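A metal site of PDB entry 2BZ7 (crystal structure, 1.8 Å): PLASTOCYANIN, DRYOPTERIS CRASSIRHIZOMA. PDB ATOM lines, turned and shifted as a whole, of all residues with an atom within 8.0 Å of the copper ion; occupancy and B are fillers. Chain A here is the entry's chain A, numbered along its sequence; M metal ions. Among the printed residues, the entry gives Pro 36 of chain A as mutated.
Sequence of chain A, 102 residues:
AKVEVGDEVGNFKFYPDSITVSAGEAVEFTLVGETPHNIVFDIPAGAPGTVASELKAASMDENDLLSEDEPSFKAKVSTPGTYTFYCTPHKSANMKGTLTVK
ND1 of His 37 sits close to SD of Met 95, 3.3 Å away.
A ring nitrogen (NE2) of His 37 lies close to the backbone carbonyl oxygen of Thr 35, 3.5 Å away.
The backbone carbonyl oxygen (O) of His 90 is in hydrogen-bond range of the backbone NH (N) of Met 95 (3.3 Å).
The backbone NH (N) of Cys 87 sits at hydrogen-bond distance from the backbone carbonyl oxygen (O) of Met 95, 3.1 Å away.
SG of Cys 87 sits close to N of Asn 38.
The backbone NH of Lys 13 sits at hydrogen-bond distance from the side-chain sulfur of Met 95, 3.6 Å away.
Pro 36 touches the copper ion (O to CU, 3.9 Å).
Of the 22 residues printed, 5 come within 4 Å of the copper ion.
The copper ion is bound by ND1 of His 37.
ND1 of His 90 binds the copper ion, 2.1 Å away.
SG of Cys 87 is bound to the copper ion, at 2.2 Å.
The copper ion has three donor atoms within binding distance.
Slightly farther from the copper ion lies the side-chain sulfur (SD) of Met 95 (2.9 Å).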
ATOM      1  N   VAL A   5     -13.837  14.088  19.024  1.00  0.00           N
ATOM      2  CA  VAL A   5     -12.448  13.669  18.911  1.00  0.00           C
ATOM      3  C   VAL A   5     -12.452  12.350  18.150  1.00  0.00           C
ATOM      4  O   VAL A   5     -12.890  11.328  18.667  1.00  0.00           O
ATOM      5  CB  VAL A   5     -11.742  13.547  20.274  1.00  0.00           C
ATOM      6  CG1 VAL A   5     -10.280  13.219  20.110  1.00  0.00           C
ATOM      7  CG2 VAL A   5     -11.927  14.829  21.130  1.00  0.00           C
ATOM      8  N   GLY A   6     -11.988  12.399  16.896  1.00  0.00           N
ATOM      9  CA  GLY A   6     -12.023  11.226  16.009  1.00  0.00           C
ATOM     10  C   GLY A   6     -13.361  11.016  15.320  1.00  0.00           C
ATOM     11  O   GLY A   6     -14.291  11.824  15.430  1.00  0.00           O
ATOM     12  N   ASN A  11     -10.322   8.347  11.102  1.00  0.00           N
ATOM     13  CA  ASN A  11      -9.526   9.535  10.782  1.00  0.00           C
ATOM     14  C   ASN A  11      -8.974  10.231  12.021  1.00  0.00           C
ATOM     15  O   ASN A  11      -9.650  10.273  13.060  1.00  0.00           O
ATOM     16  CB  ASN A  11     -10.345  10.554   9.973  1.00  0.00           C
ATOM     17  CG  ASN A  11     -10.741  10.011   8.599  1.00  0.00           C
ATOM     18  OD1 ASN A  11      -9.890   9.596   7.810  1.00  0.00           O
ATOM     19  ND2 ASN A  11     -12.029  10.012   8.310  1.00  0.00           N
ATOM     20  N   PHE A  12      -7.771  10.787  11.919  1.00  0.00           N
ATOM     21  CA  PHE A  12      -7.151  11.434  13.074  1.00  0.00           C
ATOM     22  C   PHE A  12      -7.437  12.926  13.016  1.00  0.00           C
ATOM     23  O   PHE A  12      -6.570  13.738  12.624  1.00  0.00           O
ATOM     24  CB  PHE A  12      -5.632  11.225  13.095  1.00  0.00           C
ATOM     25  CG  PHE A  12      -5.177   9.802  12.854  1.00  0.00           C
ATOM     26  CD1 PHE A  12      -5.884   8.703  13.348  1.00  0.00           C
ATOM     27  CD2 PHE A  12      -3.973   9.568  12.194  1.00  0.00           C
ATOM     28  CE1 PHE A  12      -5.402   7.387  13.104  1.00  0.00           C
ATOM     29  CE2 PHE A  12      -3.488   8.284  11.965  1.00  0.00           C
ATOM     30  CZ  PHE A  12      -4.204   7.195  12.428  1.00  0.00           C
ATOM     31  N   LYS A  13      -8.656  13.290  13.404  1.00  0.00           N
ATOM     32  CA  LYS A  13      -9.162  14.661  13.265  1.00  0.00           C
ATOM     33  C   LYS A  13     -10.045  15.014  14.424  1.00  0.00           C
ATOM     34  O   LYS A  13     -10.688  14.131  15.022  1.00  0.00           O
ATOM     35  CB  LYS A  13     -10.024  14.795  11.991  1.00  0.00           C
ATOM     36  CG  LYS A  13      -9.279  14.732  10.682  1.00  0.00           C
ATOM     37  CD  LYS A  13     -10.230  14.957   9.518  1.00  0.00           C
ATOM     38  CE  LYS A  13      -9.487  15.549   8.329  1.00  0.00           C
ATOM     39  NZ  LYS A  13      -8.879  16.844   8.771  1.00  0.00           N
ATOM     40  N   PHE A  14     -10.092  16.302  14.744  1.00  0.00           N
ATOM     41  CA  PHE A  14     -11.058  16.846  15.705  1.00  0.00           C
ATOM     42  C   PHE A  14     -12.162  17.485  14.880  1.00  0.00           C
ATOM     43  O   PHE A  14     -11.906  18.028  13.804  1.00  0.00           O
ATOM     44  CB  PHE A  14     -10.423  17.974  16.530  1.00  0.00           C
ATOM     45  CG  PHE A  14      -9.402  17.491  17.541  1.00  0.00           C
ATOM     46  CD1 PHE A  14      -9.808  17.064  18.795  1.00  0.00           C
ATOM     47  CD2 PHE A  14      -8.036  17.505  17.257  1.00  0.00           C
ATOM     48  CE1 PHE A  14      -8.863  16.635  19.743  1.00  0.00           C
ATOM     49  CE2 PHE A  14      -7.092  17.089  18.210  1.00  0.00           C
ATOM     50  CZ  PHE A  14      -7.508  16.665  19.455  1.00  0.00           C
ATOM     51  N   LEU A  31     -14.849  11.481  22.735  1.00  0.00           N
ATOM     52  CA  LEU A  31     -14.438  10.497  21.753  1.00  0.00           C
ATOM     53  C   LEU A  31     -15.591  10.014  20.869  1.00  0.00           C
ATOM     54  O   LEU A  31     -16.679   9.760  21.339  1.00  0.00           O
ATOM     55  CB  LEU A  31     -13.775   9.292  22.442  1.00  0.00           C
ATOM     56  CG  LEU A  31     -13.091   8.297  21.522  1.00  0.00           C
ATOM     57  CD1 LEU A  31     -11.857   8.972  20.987  1.00  0.00           C
ATOM     58  CD2 LEU A  31     -12.714   7.030  22.249  1.00  0.00           C
ATOM     59  N   THR A  35     -11.018   4.273  17.796  1.00  0.00           N
ATOM     60  CA  THR A  35      -9.603   4.703  17.922  1.00  0.00           C
ATOM     61  C   THR A  35      -9.435   5.648  19.151  1.00  0.00           C
ATOM     62  O   THR A  35     -10.153   6.657  19.239  1.00  0.00           O
ATOM     63  CB  THR A  35      -9.117   5.402  16.611  1.00  0.00           C
ATOM     64  OG1 THR A  35      -9.253   4.491  15.511  1.00  0.00           O
ATOM     65  CG2 THR A  35      -7.623   5.856  16.749  1.00  0.00           C
ATOM     66  N   PRO A  36      -8.528   5.319  20.105  1.00  0.00           N
ATOM     67  CA  PRO A  36      -8.251   6.219  21.245  1.00  0.00           C
ATOM     68  C   PRO A  36      -7.556   7.492  20.811  1.00  0.00           C
ATOM     69  O   PRO A  36      -6.769   7.481  19.858  1.00  0.00           O
ATOM     70  CB  PRO A  36      -7.319   5.385  22.147  1.00  0.00           C
ATOM     71  CG  PRO A  36      -7.448   3.985  21.662  1.00  0.00           C
ATOM     72  CD  PRO A  36      -7.719   4.083  20.193  1.00  0.00           C
ATOM     73  N   HIS A  37      -7.843   8.584  21.525  1.00  0.00           N
ATOM     74  CA  HIS A  37      -7.276   9.896  21.257  1.00  0.00           C
ATOM     75  C   HIS A  37      -7.154  10.607  22.590  1.00  0.00           C
ATOM     76  O   HIS A  37      -7.769  10.203  23.562  1.00  0.00           O
ATOM     77  CB  HIS A  37      -8.212  10.721  20.335  1.00  0.00           C
ATOM     78  CG  HIS A  37      -8.421  10.139  18.960  1.00  0.00           C
ATOM     79  ND1 HIS A  37      -7.413  10.053  18.025  1.00  0.00           N
ATOM     80  CD2 HIS A  37      -9.522   9.620  18.364  1.00  0.00           C
ATOM     81  CE1 HIS A  37      -7.873   9.502  16.927  1.00  0.00           C
ATOM     82  NE2 HIS A  37      -9.149   9.217  17.100  1.00  0.00           N
ATOM     83  N   ASN A  38      -6.386  11.679  22.623  1.00  0.00           N
ATOM     84  CA  ASN A  38      -6.417  12.581  23.765  1.00  0.00           C
ATOM     85  C   ASN A  38      -6.393  14.028  23.265  1.00  0.00           C
ATOM     86  O   ASN A  38      -6.503  14.274  22.047  1.00  0.00           O
ATOM     87  CB  ASN A  38      -5.319  12.210  24.792  1.00  0.00           C
ATOM     88  CG  ASN A  38      -3.946  12.713  24.414  1.00  0.00           C
ATOM     89  OD1 ASN A  38      -3.726  13.220  23.306  1.00  0.00           O
ATOM     90  ND2 ASN A  38      -3.008  12.580  25.349  1.00  0.00           N
ATOM     91  N   ILE A  39      -6.299  14.978  24.202  1.00  0.00           N
ATOM     92  CA  ILE A  39      -6.140  16.364  23.816  1.00  0.00           C
ATOM     93  C   ILE A  39      -5.218  17.057  24.786  1.00  0.00           C
ATOM     94  O   ILE A  39      -5.370  16.915  25.977  1.00  0.00           O
ATOM     95  CB  ILE A  39      -7.513  17.050  23.654  1.00  0.00           C
ATOM     96  CG1 ILE A  39      -7.414  18.515  23.203  1.00  0.00           C
ATOM     97  CG2 ILE A  39      -8.436  16.804  24.916  1.00  0.00           C
ATOM     98  CD1 ILE A  39      -7.247  19.505  24.321  1.00  0.00           C
ATOM     99  N   LEU A  65      -5.556   8.437  27.640  1.00  0.00           N
ATOM    100  CA  LEU A  65      -6.338   8.416  26.420  1.00  0.00           C
ATOM    101  C   LEU A  65      -7.817   8.367  26.742  1.00  0.00           C
ATOM    102  O   LEU A  65      -8.222   7.736  27.715  1.00  0.00           O
ATOM    103  CB  LEU A  65      -5.942   7.228  25.526  1.00  0.00           C
ATOM    104  CG  LEU A  65      -4.522   7.217  24.955  1.00  0.00           C
ATOM    105  CD1 LEU A  65      -4.167   5.857  24.336  1.00  0.00           C
ATOM    106  CD2 LEU A  65      -4.309   8.325  23.969  1.00  0.00           C
ATOM    107  N   TYR A  86      -3.408  19.506  20.397  1.00  0.00           N
ATOM    108  CA  TYR A  86      -3.136  18.333  19.566  1.00  0.00           C
ATOM    109  C   TYR A  86      -3.520  17.029  20.302  1.00  0.00           C
ATOM    110  O   TYR A  86      -3.743  17.036  21.529  1.00  0.00           O
ATOM    111  CB  TYR A  86      -1.645  18.351  19.143  1.00  0.00           C
ATOM    112  CG  TYR A  86      -0.699  18.288  20.311  1.00  0.00           C
ATOM    113  CD1 TYR A  86      -0.272  17.066  20.832  1.00  0.00           C
ATOM    114  CD2 TYR A  86      -0.240  19.470  20.925  1.00  0.00           C
ATOM    115  CE1 TYR A  86       0.629  17.026  21.926  1.00  0.00           C
ATOM    116  CE2 TYR A  86       0.628  19.427  22.001  1.00  0.00           C
ATOM    117  CZ  TYR A  86       1.057  18.212  22.499  1.00  0.00           C
ATOM    118  OH  TYR A  86       1.914  18.208  23.566  1.00  0.00           O
ATOM    119  N   CYS A  87      -3.617  15.935  19.545  1.00  0.00           N
ATOM    120  CA  CYS A  87      -3.678  14.589  20.093  1.00  0.00           C
ATOM    121  C   CYS A  87      -2.269  14.006  20.160  1.00  0.00           C
ATOM    122  O   CYS A  87      -1.617  13.937  19.130  1.00  0.00           O
ATOM    123  CB  CYS A  87      -4.550  13.697  19.189  1.00  0.00           C
ATOM    124  SG  CYS A  87      -4.482  11.970  19.716  1.00  0.00           S
ATOM    125  N   THR A  88      -1.820  13.582  21.349  1.00  0.00           N
ATOM    126  CA  THR A  88      -0.479  12.989  21.562  1.00  0.00           C
ATOM    127  C   THR A  88      -0.128  11.848  20.589  1.00  0.00           C
ATOM    128  O   THR A  88       0.843  11.965  19.842  1.00  0.00           O
ATOM    129  CB  THR A  88      -0.287  12.520  23.050  1.00  0.00           C
ATOM    130  OG1 THR A  88      -0.324  13.659  23.914  1.00  0.00           O
ATOM    131  CG2 THR A  88       1.031  11.755  23.257  1.00  0.00           C
ATOM    132  N   PRO A  89      -0.893  10.738  20.600  1.00  0.00           N
ATOM    133  CA  PRO A  89      -0.489   9.681  19.653  1.00  0.00           C
ATOM    134  C   PRO A  89      -0.465  10.070  18.176  1.00  0.00           C
ATOM    135  O   PRO A  89       0.448   9.632  17.464  1.00  0.00           O
ATOM    136  CB  PRO A  89      -1.511   8.559  19.892  1.00  0.00           C
ATOM    137  CG  PRO A  89      -2.603   9.160  20.661  1.00  0.00           C
ATOM    138  CD  PRO A  89      -2.022  10.301  21.442  1.00  0.00           C
ATOM    139  N   HIS A  90      -1.410  10.891  17.724  1.00  0.00           N
ATOM    140  CA  HIS A  90      -1.520  11.273  16.306  1.00  0.00           C
ATOM    141  C   HIS A  90      -0.981  12.668  15.947  1.00  0.00           C
ATOM    142  O   HIS A  90      -1.321  13.223  14.897  1.00  0.00           O
ATOM    143  CB  HIS A  90      -2.930  11.062  15.805  1.00  0.00           C
ATOM    144  CG  HIS A  90      -3.437   9.665  16.023  1.00  0.00           C
ATOM    145  ND1 HIS A  90      -4.420   9.356  16.936  1.00  0.00           N
ATOM    146  CD2 HIS A  90      -3.039   8.478  15.499  1.00  0.00           C
ATOM    147  CE1 HIS A  90      -4.638   8.061  16.936  1.00  0.00           C
ATOM    148  NE2 HIS A  90      -3.815   7.500  16.063  1.00  0.00           N
ATOM    149  N   LYS A  91      -0.099  13.207  16.789  1.00  0.00           N
ATOM    150  CA  LYS A  91       0.464  14.551  16.602  1.00  0.00           C
ATOM    151  C   LYS A  91       1.187  14.733  15.272  1.00  0.00           C
ATOM    152  O   LYS A  91       0.991  15.729  14.559  1.00  0.00           O
ATOM    153  CB  LYS A  91       1.364  14.912  17.770  1.00  0.00           C
ATOM    154  CG  LYS A  91       1.741  16.375  17.815  1.00  0.00           C
ATOM    155  CD  LYS A  91       2.768  16.619  18.911  1.00  0.00           C
ATOM    156  CE  LYS A  91       2.942  18.106  19.174  1.00  0.00           C
ATOM    157  NZ  LYS A  91       3.692  18.751  18.069  1.00  0.00           N
ATOM    158  N   ALA A  93       0.570  13.033  12.689  1.00  0.00           N
ATOM    159  CA  ALA A  93      -0.461  12.869  11.664  1.00  0.00           C
ATOM    160  C   ALA A  93      -1.337  14.111  11.545  1.00  0.00           C
ATOM    161  O   ALA A  93      -2.381  14.100  10.879  1.00  0.00           O
ATOM    162  CB  ALA A  93      -1.311  11.634  11.958  1.00  0.00           C
ATOM    163  N   MET A  95      -3.066  15.820  13.747  1.00  0.00           N
ATOM    164  CA  MET A  95      -4.323  15.793  14.481  1.00  0.00           C
ATOM    165  C   MET A  95      -4.316  16.936  15.472  1.00  0.00           C
ATOM    166  O   MET A  95      -3.781  16.811  16.591  1.00  0.00           O
ATOM    167  CB  MET A  95      -4.529  14.449  15.193  1.00  0.00           C
ATOM    168  CG  MET A  95      -5.894  14.377  15.866  1.00  0.00           C
ATOM    169  SD  MET A  95      -6.522  12.747  16.304  1.00  0.00           S
ATOM    170  CE  MET A  95      -7.963  13.269  17.259  1.00  0.00           C
ATOM    171  N   LYS A  96      -4.910  18.058  15.081  1.00  0.00           N
ATOM    172  CA  LYS A  96      -4.760  19.285  15.855  1.00  0.00           C
ATOM    173  C   LYS A  96      -5.936  20.180  15.646  1.00  0.00           C
ATOM    174  O   LYS A  96      -6.707  19.999  14.696  1.00  0.00           O
ATOM    175  CB  LYS A  96      -3.434  20.012  15.538  1.00  0.00           C
ATOM    176  CG  LYS A  96      -3.195  20.554  14.135  1.00  0.00           C
ATOM    177  CD  LYS A  96      -1.695  20.543  13.907  1.00  0.00           C
ATOM    178  CE  LYS A  96      -1.161  21.771  13.094  1.00  0.00           C
ATOM    179  NZ  LYS A  96      -1.166  22.988  14.018  1.00  0.00           N
HETATM  180 CU    CU M   1      -5.460  10.790  18.145  1.00  0.00          CU
